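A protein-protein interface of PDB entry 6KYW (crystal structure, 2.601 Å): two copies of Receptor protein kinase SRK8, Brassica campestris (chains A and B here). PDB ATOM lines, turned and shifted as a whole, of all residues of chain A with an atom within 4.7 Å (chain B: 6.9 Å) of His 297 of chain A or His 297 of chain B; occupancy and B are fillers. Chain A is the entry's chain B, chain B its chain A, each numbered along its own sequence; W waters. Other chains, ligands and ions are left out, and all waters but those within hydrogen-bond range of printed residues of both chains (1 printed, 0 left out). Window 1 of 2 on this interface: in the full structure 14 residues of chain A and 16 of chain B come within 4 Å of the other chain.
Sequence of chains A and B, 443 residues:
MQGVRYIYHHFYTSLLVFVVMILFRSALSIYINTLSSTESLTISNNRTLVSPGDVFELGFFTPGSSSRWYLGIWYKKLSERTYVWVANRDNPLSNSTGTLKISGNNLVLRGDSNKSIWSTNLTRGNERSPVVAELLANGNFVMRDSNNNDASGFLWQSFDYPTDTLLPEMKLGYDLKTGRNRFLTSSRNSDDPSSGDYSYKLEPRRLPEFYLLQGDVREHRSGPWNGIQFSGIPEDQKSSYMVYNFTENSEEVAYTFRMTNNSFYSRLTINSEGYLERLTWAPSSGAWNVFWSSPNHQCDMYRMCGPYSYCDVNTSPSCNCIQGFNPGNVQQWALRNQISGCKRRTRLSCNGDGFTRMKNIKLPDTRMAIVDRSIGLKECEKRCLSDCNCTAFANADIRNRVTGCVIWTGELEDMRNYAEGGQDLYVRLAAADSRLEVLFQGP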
ATOM      1  N   PRO A 295      -4.261  -5.614 -13.147  1.00  0.00           N
ATOM      2  CA  PRO A 295      -4.975  -6.746 -12.534  1.00  0.00           C
ATOM      3  C   PRO A 295      -5.130  -6.551 -11.026  1.00  0.00           C
ATOM      4  O   PRO A 295      -4.373  -5.780 -10.446  1.00  0.00           O
ATOM      5  CB  PRO A 295      -4.045  -7.924 -12.826  1.00  0.00           C
ATOM      6  CG  PRO A 295      -2.677  -7.299 -12.798  1.00  0.00           C
ATOM      7  CD  PRO A 295      -2.866  -5.961 -13.485  1.00  0.00           C
ATOM      8  N   ASN A 296      -6.058  -7.228 -10.374  1.00  0.00           N
ATOM      9  CA  ASN A 296      -6.140  -7.062  -8.928  1.00  0.00           C
ATOM     10  C   ASN A 296      -6.337  -8.382  -8.191  1.00  0.00           C
ATOM     11  O   ASN A 296      -6.773  -8.380  -7.031  1.00  0.00           O
ATOM     12  CB  ASN A 296      -7.247  -6.070  -8.551  1.00  0.00           C
ATOM     13  CG  ASN A 296      -8.611  -6.580  -8.898  1.00  0.00           C
ATOM     14  OD1 ASN A 296      -9.221  -7.314  -8.120  1.00  0.00           O
ATOM     15  ND2 ASN A 296      -9.113  -6.194 -10.074  1.00  0.00           N
ATOM     16  N   HIS A 297      -6.023  -9.505  -8.831  1.00  0.00           N
ATOM     17  CA  HIS A 297      -6.058 -10.816  -8.196  1.00  0.00           C
ATOM     18  C   HIS A 297      -5.046 -11.687  -8.928  1.00  0.00           C
ATOM     19  O   HIS A 297      -4.756 -11.448 -10.108  1.00  0.00           O
ATOM     20  CB  HIS A 297      -7.481 -11.413  -8.237  1.00  0.00           C
ATOM     21  CG  HIS A 297      -7.648 -12.648  -7.409  1.00  0.00           C
ATOM     22  ND1 HIS A 297      -6.887 -13.783  -7.600  1.00  0.00           N
ATOM     23  CD2 HIS A 297      -8.496 -12.933  -6.391  1.00  0.00           C
ATOM     24  CE1 HIS A 297      -7.261 -14.712  -6.739  1.00  0.00           C
ATOM     25  NE2 HIS A 297      -8.233 -14.221  -5.992  1.00  0.00           N
ATOM     26  N   GLN A 298      -4.469 -12.666  -8.223  1.00  0.00           N
ATOM     27  CA  GLN A 298      -3.530 -13.561  -8.907  1.00  0.00           C
ATOM     28  C   GLN A 298      -4.233 -14.347 -10.020  1.00  0.00           C
ATOM     29  O   GLN A 298      -3.610 -14.664 -11.044  1.00  0.00           O
ATOM     30  CB  GLN A 298      -2.857 -14.500  -7.909  1.00  0.00           C
ATOM     31  CG  GLN A 298      -2.471 -13.801  -6.620  1.00  0.00           C
ATOM     32  CD  GLN A 298      -1.915 -14.745  -5.570  1.00  0.00           C
ATOM     33  OE1 GLN A 298      -2.606 -15.659  -5.099  1.00  0.00           O
ATOM     34  NE2 GLN A 298      -0.669 -14.513  -5.177  1.00  0.00           N
ATOM     35  N   CYS A 299      -5.540 -14.606  -9.867  1.00  0.00           N
ATOM     36  CA  CYS A 299      -6.330 -15.206 -10.939  1.00  0.00           C
ATOM     37  C   CYS A 299      -6.401 -14.323 -12.174  1.00  0.00           C
ATOM     38  O   CYS A 299      -6.839 -14.800 -13.221  1.00  0.00           O
ATOM     39  CB  CYS A 299      -7.754 -15.523 -10.455  1.00  0.00           C
ATOM     40  SG  CYS A 299      -7.792 -16.984  -9.328  1.00  0.00           S
ATOM     41  N   ASP A 300      -6.044 -13.037 -12.071  1.00  0.00           N
ATOM     42  CA  ASP A 300      -5.940 -12.196 -13.253  1.00  0.00           C
ATOM     43  C   ASP A 300      -4.555 -12.227 -13.846  1.00  0.00           C
ATOM     44  O   ASP A 300      -4.326 -11.581 -14.870  1.00  0.00           O
ATOM     45  CB  ASP A 300      -6.261 -10.726 -12.943  1.00  0.00           C
ATOM     46  CG  ASP A 300      -7.693 -10.501 -12.545  1.00  0.00           C
ATOM     47  OD1 ASP A 300      -8.509 -11.444 -12.645  1.00  0.00           O
ATOM     48  OD2 ASP A 300      -7.996  -9.365 -12.118  1.00  0.00           O
ATOM     49  N   MET A 301      -3.608 -12.896 -13.200  1.00  0.00           N
ATOM     50  CA  MET A 301      -2.274 -12.928 -13.766  1.00  0.00           C
ATOM     51  C   MET A 301      -2.228 -13.955 -14.886  1.00  0.00           C
ATOM     52  O   MET A 301      -2.836 -15.031 -14.798  1.00  0.00           O
ATOM     53  CB  MET A 301      -1.238 -13.209 -12.676  1.00  0.00           C
ATOM     54  CG  MET A 301      -1.137 -12.083 -11.629  1.00  0.00           C
ATOM     55  SD  MET A 301      -0.789 -10.466 -12.246  1.00  0.00           S
ATOM     56  CE  MET A 301       0.896 -10.725 -12.683  1.00  0.00           C
ATOM     57  N   VAL A 313     -11.229 -17.589  -7.453  1.00  0.00           N
ATOM     58  CA  VAL A 313     -10.874 -16.816  -6.268  1.00  0.00           C
ATOM     59  C   VAL A 313     -11.543 -17.328  -4.995  1.00  0.00           C
ATOM     60  O   VAL A 313     -11.112 -16.963  -3.902  1.00  0.00           O
ATOM     61  CB  VAL A 313     -11.180 -15.324  -6.517  1.00  0.00           C
ATOM     62  CG1 VAL A 313     -10.678 -14.934  -7.897  1.00  0.00           C
ATOM     63  CG2 VAL A 313     -12.683 -15.022  -6.355  1.00  0.00           C
ATOM     64  N   ARG A 416     -10.252 -17.812 -15.841  1.00  0.00           N
ATOM     65  CA  ARG A 416     -10.690 -17.657 -14.470  1.00  0.00           C
ATOM     66  C   ARG A 416     -12.198 -17.524 -14.525  1.00  0.00           C
ATOM     67  O   ARG A 416     -12.767 -17.229 -15.581  1.00  0.00           O
ATOM     68  CB  ARG A 416     -10.018 -16.440 -13.810  1.00  0.00           C
ATOM     69  CG  ARG A 416     -10.559 -15.121 -14.359  1.00  0.00           C
ATOM     70  CD  ARG A 416     -10.374 -13.999 -13.387  1.00  0.00           C
ATOM     71  NE  ARG A 416     -11.387 -14.038 -12.348  1.00  0.00           N
ATOM     72  CZ  ARG A 416     -11.383 -13.255 -11.266  1.00  0.00           C
ATOM     73  NH1 ARG A 416     -10.419 -12.363 -11.080  1.00  0.00           N
ATOM     74  NH2 ARG A 416     -12.348 -13.373 -10.359  1.00  0.00           N
ATOM     75  N   HIS B 220      -0.231  -6.449   6.829  1.00  0.00           N
ATOM     76  CA  HIS B 220      -1.133  -7.591   6.827  1.00  0.00           C
ATOM     77  C   HIS B 220      -1.196  -8.157   8.247  1.00  0.00           C
ATOM     78  O   HIS B 220      -0.250  -8.007   9.027  1.00  0.00           O
ATOM     79  CB  HIS B 220      -0.647  -8.645   5.799  1.00  0.00           C
ATOM     80  CG  HIS B 220      -1.191 -10.013   6.040  1.00  0.00           C
ATOM     81  ND1 HIS B 220      -2.492 -10.357   5.743  1.00  0.00           N
ATOM     82  CD2 HIS B 220      -0.630 -11.109   6.605  1.00  0.00           C
ATOM     83  CE1 HIS B 220      -2.709 -11.606   6.113  1.00  0.00           C
ATOM     84  NE2 HIS B 220      -1.594 -12.086   6.635  1.00  0.00           N
ATOM     85  N   TYR B 275       6.325 -11.569   1.513  1.00  0.00           N
ATOM     86  CA  TYR B 275       5.263 -12.561   1.551  1.00  0.00           C
ATOM     87  C   TYR B 275       5.707 -13.690   2.463  1.00  0.00           C
ATOM     88  O   TYR B 275       6.862 -14.131   2.398  1.00  0.00           O
ATOM     89  CB  TYR B 275       4.922 -13.099   0.154  1.00  0.00           C
ATOM     90  CG  TYR B 275       4.382 -12.067  -0.827  1.00  0.00           C
ATOM     91  CD1 TYR B 275       5.247 -11.325  -1.608  1.00  0.00           C
ATOM     92  CD2 TYR B 275       2.994 -11.840  -0.965  1.00  0.00           C
ATOM     93  CE1 TYR B 275       4.776 -10.380  -2.499  1.00  0.00           C
ATOM     94  CE2 TYR B 275       2.505 -10.895  -1.861  1.00  0.00           C
ATOM     95  CZ  TYR B 275       3.419 -10.173  -2.641  1.00  0.00           C
ATOM     96  OH  TYR B 275       3.004  -9.218  -3.557  1.00  0.00           O
ATOM     97  N   SER B 293       0.996 -18.713  -0.010  1.00  0.00           N
ATOM     98  CA  SER B 293       1.574 -17.377   0.017  1.00  0.00           C
ATOM     99  C   SER B 293       0.622 -16.448   0.772  1.00  0.00           C
ATOM    100  O   SER B 293      -0.599 -16.559   0.647  1.00  0.00           O
ATOM    101  CB  SER B 293       1.817 -16.880  -1.410  1.00  0.00           C
ATOM    102  OG  SER B 293       2.630 -15.726  -1.444  1.00  0.00           O
ATOM    103  N   SER B 294       1.177 -15.546   1.576  1.00  0.00           N
ATOM    104  CA  SER B 294       0.361 -14.650   2.392  1.00  0.00           C
ATOM    105  C   SER B 294       1.108 -13.339   2.606  1.00  0.00           C
ATOM    106  O   SER B 294       2.323 -13.368   2.901  1.00  0.00           O
ATOM    107  CB  SER B 294       0.026 -15.292   3.731  1.00  0.00           C
ATOM    108  OG  SER B 294      -1.212 -14.835   4.212  1.00  0.00           O
ATOM    109  N   PRO B 295       0.446 -12.187   2.412  1.00  0.00           N
ATOM    110  CA  PRO B 295      -0.922 -12.086   1.893  1.00  0.00           C
ATOM    111  C   PRO B 295      -0.953 -12.353   0.395  1.00  0.00           C
ATOM    112  O   PRO B 295       0.087 -12.203  -0.249  1.00  0.00           O
ATOM    113  CB  PRO B 295      -1.283 -10.624   2.163  1.00  0.00           C
ATOM    114  CG  PRO B 295       0.039  -9.913   1.907  1.00  0.00           C
ATOM    115  CD  PRO B 295       1.098 -10.862   2.481  1.00  0.00           C
ATOM    116  N   ASN B 296      -2.103 -12.687  -0.177  1.00  0.00           N
ATOM    117  CA  ASN B 296      -2.146 -12.933  -1.613  1.00  0.00           C
ATOM    118  C   ASN B 296      -3.131 -12.049  -2.371  1.00  0.00           C
ATOM    119  O   ASN B 296      -3.122 -12.080  -3.612  1.00  0.00           O
ATOM    120  CB  ASN B 296      -2.438 -14.418  -1.893  1.00  0.00           C
ATOM    121  CG  ASN B 296      -3.690 -14.885  -1.231  1.00  0.00           C
ATOM    122  OD1 ASN B 296      -4.734 -14.239  -1.331  1.00  0.00           O
ATOM    123  ND2 ASN B 296      -3.595 -15.989  -0.502  1.00  0.00           N
ATOM    124  N   HIS B 297      -3.952 -11.250  -1.672  1.00  0.00           N
ATOM    125  CA  HIS B 297      -4.924 -10.343  -2.285  1.00  0.00           C
ATOM    126  C   HIS B 297      -5.026  -9.028  -1.515  1.00  0.00           C
ATOM    127  O   HIS B 297      -4.790  -8.970  -0.305  1.00  0.00           O
ATOM    128  CB  HIS B 297      -6.327 -10.943  -2.351  1.00  0.00           C
ATOM    129  CG  HIS B 297      -7.249 -10.167  -3.239  1.00  0.00           C
ATOM    130  ND1 HIS B 297      -8.374  -9.515  -2.776  1.00  0.00           N
ATOM    131  CD2 HIS B 297      -7.179  -9.900  -4.563  1.00  0.00           C
ATOM    132  CE1 HIS B 297      -8.965  -8.901  -3.784  1.00  0.00           C
ATOM    133  NE2 HIS B 297      -8.253  -9.111  -4.878  1.00  0.00           N
ATOM    134  N   GLN B 298      -5.453  -7.969  -2.217  1.00  0.00           N
ATOM    135  CA  GLN B 298      -5.644  -6.687  -1.542  1.00  0.00           C
ATOM    136  C   GLN B 298      -6.618  -6.805  -0.373  1.00  0.00           C
ATOM    137  O   GLN B 298      -6.471  -6.095   0.624  1.00  0.00           O
ATOM    138  CB  GLN B 298      -6.122  -5.626  -2.527  1.00  0.00           C
ATOM    139  CG  GLN B 298      -7.589  -5.747  -2.886  1.00  0.00           C
ATOM    140  CD  GLN B 298      -8.013  -4.728  -3.906  1.00  0.00           C
ATOM    141  OE1 GLN B 298      -8.918  -3.914  -3.654  1.00  0.00           O
ATOM    142  NE2 GLN B 298      -7.360  -4.755  -5.069  1.00  0.00           N
ATOM    143  N   CYS B 299      -7.575  -7.734  -0.441  1.00  0.00           N
ATOM    144  CA  CYS B 299      -8.503  -7.959   0.665  1.00  0.00           C
ATOM    145  C   CYS B 299      -7.852  -8.613   1.853  1.00  0.00           C
ATOM    146  O   CYS B 299      -8.564  -8.953   2.800  1.00  0.00           O
ATOM    147  CB  CYS B 299      -9.673  -8.832   0.217  1.00  0.00           C
ATOM    148  SG  CYS B 299     -11.070  -7.907  -0.509  1.00  0.00           S
ATOM    149  N   ASP B 300      -6.551  -8.888   1.766  1.00  0.00           N
ATOM    150  CA  ASP B 300      -5.722  -9.388   2.852  1.00  0.00           C
ATOM    151  C   ASP B 300      -4.827  -8.296   3.415  1.00  0.00           C
ATOM    152  O   ASP B 300      -4.144  -8.528   4.416  1.00  0.00           O
ATOM    153  CB  ASP B 300      -4.800 -10.527   2.362  1.00  0.00           C
ATOM    154  CG  ASP B 300      -5.490 -11.861   2.238  1.00  0.00           C
ATOM    155  OD1 ASP B 300      -6.518 -12.098   2.913  1.00  0.00           O
ATOM    156  OD2 ASP B 300      -4.953 -12.701   1.476  1.00  0.00           O
ATOM    157  N   MET B 301      -4.723  -7.168   2.717  1.00  0.00           N
ATOM    158  CA  MET B 301      -3.922  -6.055   3.190  1.00  0.00           C
ATOM    159  C   MET B 301      -4.650  -5.363   4.332  1.00  0.00           C
ATOM    160  O   MET B 301      -5.885  -5.356   4.400  1.00  0.00           O
ATOM    161  CB  MET B 301      -3.647  -5.076   2.056  1.00  0.00           C
ATOM    162  CG  MET B 301      -2.940  -5.689   0.867  1.00  0.00           C
ATOM    163  SD  MET B 301      -1.357  -6.411   1.345  1.00  0.00           S
ATOM    164  CE  MET B 301      -0.335  -4.945   1.528  1.00  0.00           C
ATOM    165  N   MET B 304      -7.875  -2.742   4.221  1.00  0.00           N
ATOM    166  CA  MET B 304      -8.228  -2.423   2.849  1.00  0.00           C
ATOM    167  C   MET B 304      -9.617  -1.808   2.795  1.00  0.00           C
ATOM    168  O   MET B 304      -9.912  -1.014   1.893  1.00  0.00           O
ATOM    169  CB  MET B 304      -8.148  -3.678   1.974  1.00  0.00           C
ATOM    170  CG  MET B 304      -8.325  -3.414   0.485  1.00  0.00           C
ATOM    171  SD  MET B 304      -6.918  -2.547  -0.225  1.00  0.00           S
ATOM    172  CE  MET B 304      -7.609  -0.907  -0.524  1.00  0.00           C
ATOM    173  N   CYS B 311     -14.005  -6.583   3.417  1.00  0.00           N
ATOM    174  CA  CYS B 311     -13.513  -6.740   2.059  1.00  0.00           C
ATOM    175  C   CYS B 311     -13.994  -8.076   1.483  1.00  0.00           C
ATOM    176  O   CYS B 311     -14.144  -9.062   2.212  1.00  0.00           O
ATOM    177  CB  CYS B 311     -11.992  -6.638   2.072  1.00  0.00           C
ATOM    178  SG  CYS B 311     -11.222  -6.142   0.508  1.00  0.00           S
ATOM    179  N   ASP B 312     -14.299  -8.086   0.176  1.00  0.00           N
ATOM    180  CA  ASP B 312     -14.796  -9.270  -0.525  1.00  0.00           C
ATOM    181  C   ASP B 312     -14.095  -9.366  -1.875  1.00  0.00           C
ATOM    182  O   ASP B 312     -14.056  -8.374  -2.614  1.00  0.00           O
ATOM    183  CB  ASP B 312     -16.317  -9.202  -0.726  1.00  0.00           C
ATOM    184  CG  ASP B 312     -16.918 -10.537  -1.175  1.00  0.00           C
ATOM    185  OD1 ASP B 312     -16.329 -11.190  -2.070  1.00  0.00           O
ATOM    186  OD2 ASP B 312     -17.979 -10.936  -0.633  1.00  0.00           O
ATOM    187  N   VAL B 313     -13.542 -10.550  -2.198  1.00  0.00           N
ATOM    188  CA  VAL B 313     -12.860 -10.716  -3.490  1.00  0.00           C
ATOM    189  C   VAL B 313     -13.858 -10.800  -4.640  1.00  0.00           C
ATOM    190  O   VAL B 313     -13.481 -10.565  -5.789  1.00  0.00           O
ATOM    191  CB  VAL B 313     -11.915 -11.947  -3.570  1.00  0.00           C
ATOM    192  CG1 VAL B 313     -10.560 -11.700  -2.883  1.00  0.00           C
ATOM    193  CG2 VAL B 313     -12.589 -13.243  -3.089  1.00  0.00           C
ATOM    194  N   ASN B 314     -15.130 -11.084  -4.355  1.00  0.00           N
ATOM    195  CA  ASN B 314     -16.163 -11.233  -5.367  1.00  0.00           C
ATOM    196  C   ASN B 314     -16.917  -9.952  -5.725  1.00  0.00           C
ATOM    197  O   ASN B 314     -17.862 -10.027  -6.517  1.00  0.00           O
ATOM    198  CB  ASN B 314     -17.197 -12.261  -4.902  1.00  0.00           C
ATOM    199  CG  ASN B 314     -16.688 -13.667  -4.985  1.00  0.00           C
ATOM    200  OD1 ASN B 314     -16.781 -14.426  -4.015  1.00  0.00           O
ATOM    201  ND2 ASN B 314     -16.147 -14.039  -6.153  1.00  0.00           N
ATOM    202  N   SER B 318     -14.576  -3.537  -3.472  1.00  0.00           N
ATOM    203  CA  SER B 318     -14.311  -4.615  -2.517  1.00  0.00           C
ATOM    204  C   SER B 318     -15.145  -4.471  -1.255  1.00  0.00           C
ATOM    205  O   SER B 318     -15.700  -5.461  -0.756  1.00  0.00           O
ATOM    206  CB  SER B 318     -12.829  -4.647  -2.146  1.00  0.00           C
ATOM    207  OG  SER B 318     -11.986  -4.315  -3.242  1.00  0.00           O
ATOM    208  N   ARG B 416     -12.719  -9.285   6.421  1.00  0.00           N
ATOM    209  CA  ARG B 416     -12.880  -9.781   5.063  1.00  0.00           C
ATOM    210  C   ARG B 416     -13.615 -11.092   5.187  1.00  0.00           C
ATOM    211  O   ARG B 416     -13.549 -11.738   6.239  1.00  0.00           O
ATOM    212  CB  ARG B 416     -11.541  -9.963   4.355  1.00  0.00           C
ATOM    213  CG  ARG B 416     -10.662 -11.071   4.942  1.00  0.00           C
ATOM    214  CD  ARG B 416      -9.766 -11.695   3.885  1.00  0.00           C
ATOM    215  NE  ARG B 416     -10.551 -12.481   2.928  1.00  0.00           N
ATOM    216  CZ  ARG B 416     -10.067 -13.029   1.815  1.00  0.00           C
ATOM    217  NH1 ARG B 416      -8.787 -12.896   1.508  1.00  0.00           N
ATOM    218  NH2 ARG B 416     -10.868 -13.721   1.011  1.00  0.00           N
HETATM  219  O   HOH W   1      -2.328 -17.614  -3.085  1.00  0.00           O
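A ring nitrogen (NE2) of His 297 of chain B lies within hydrogen-bond range of the backbone carbonyl oxygen (O) of Asn 296 of chain A (2.7 Å).
The backbone carbonyl oxygen of Ser 293 of chain B lies within hydrogen-bond range of the side-chain amide nitrogen of Asn 296 of chain B.
The side-chain carboxylate (OD2) of Asp 300 of chain B lies close to the side-chain amide oxygen (OD1) of Asn 296 of chain B (3.2 Å).
The backbone NH (N) of Cys 299 of chain B lies within hydrogen-bond range of a ring nitrogen (ND1) of His 297 of chain B (3.0 Å).
OD1 of Asp 312 of chain B lies within hydrogen-bond range of N of Asn 314 of chain B, at 2.6 Å.
N of Asn 296 of chain A lies within hydrogen-bond range of OD2 of Asp 300 of chain A (3.4 Å).
A ring nitrogen (ND1) of His 297 of chain A sits at hydrogen-bond distance from the backbone NH of Cys 299 of chain A (2.8 Å).
Asn 296 of chain A touches Gln 298 of chain B (CB to NE2, 3.7 Å).
His 297 of chain A touches His 297 of chain B (CD2 to CD2, 3.8 Å).
CB of Asn 296 of chain B touches OE1 of Gln 298 of chain A, at 3.4 Å.
Val 313 of chain A touches Val 313 of chain B (CG2 to CG2, 3.7 Å).
Asn 314 of chain B touches Val 313 of chain A.
His 297 of chain B touches two residues of chain A.
Printed residues of chain B within 4 Å of Asn 296 of chain A: His 297 and Gln 298.
Printed residues of chain A within 4 Å of Asn 296 of chain B: Gln 298 (3.4 Å).
Printed residues of chain A within 4 Å of Val 313 of chain B: Val 313.
Printed residues of chain B within 4 Å of Val 313 of chain A: Val 313 and Asn 314.
Printed residues of chain B within 4 Å of Gln 298 of chain A: Asn 296.
Cys 311 of chain B touches none of the printed residues of chain A.
Hydrophobic or aromatic side chains of chain A that line the printed part of chain B: His 297 and Val 313.
Along chain A the printed residues that touch a printed residue of chain B span positions 296 to 313.
Of the 18 printed residues of chain B, 5 touch a printed residue of chain A.
Hydrophobic or aromatic side chains of chain B that line the printed part of chain A: His 297 and Val 313.
Among the printed residues, no Asp or Glu carboxylate lies within 4 Å of a Lys or Arg side-chain nitrogen of the other chain.
Asn 296 of chain A touches His 297 of chain B, but with the chains exchanged His 297 of chain A does not touch Asn 296 of chain B (5.6 Å).
Asn 296 of chain A touches Gln 298 of chain B, and with the chains exchanged Gln 298 of chain A touches Asn 296 of chain B.
His 297 of chain B touches its own counterpart, His 297 of chain A.
Val 313 of chain A touches its own counterpart, Val 313 of chain B.
Water W1 bridges OE1 of Gln 298 of chain A (2.8 Å) and ND2 of Asn 296 of chain B (3.3 Å).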
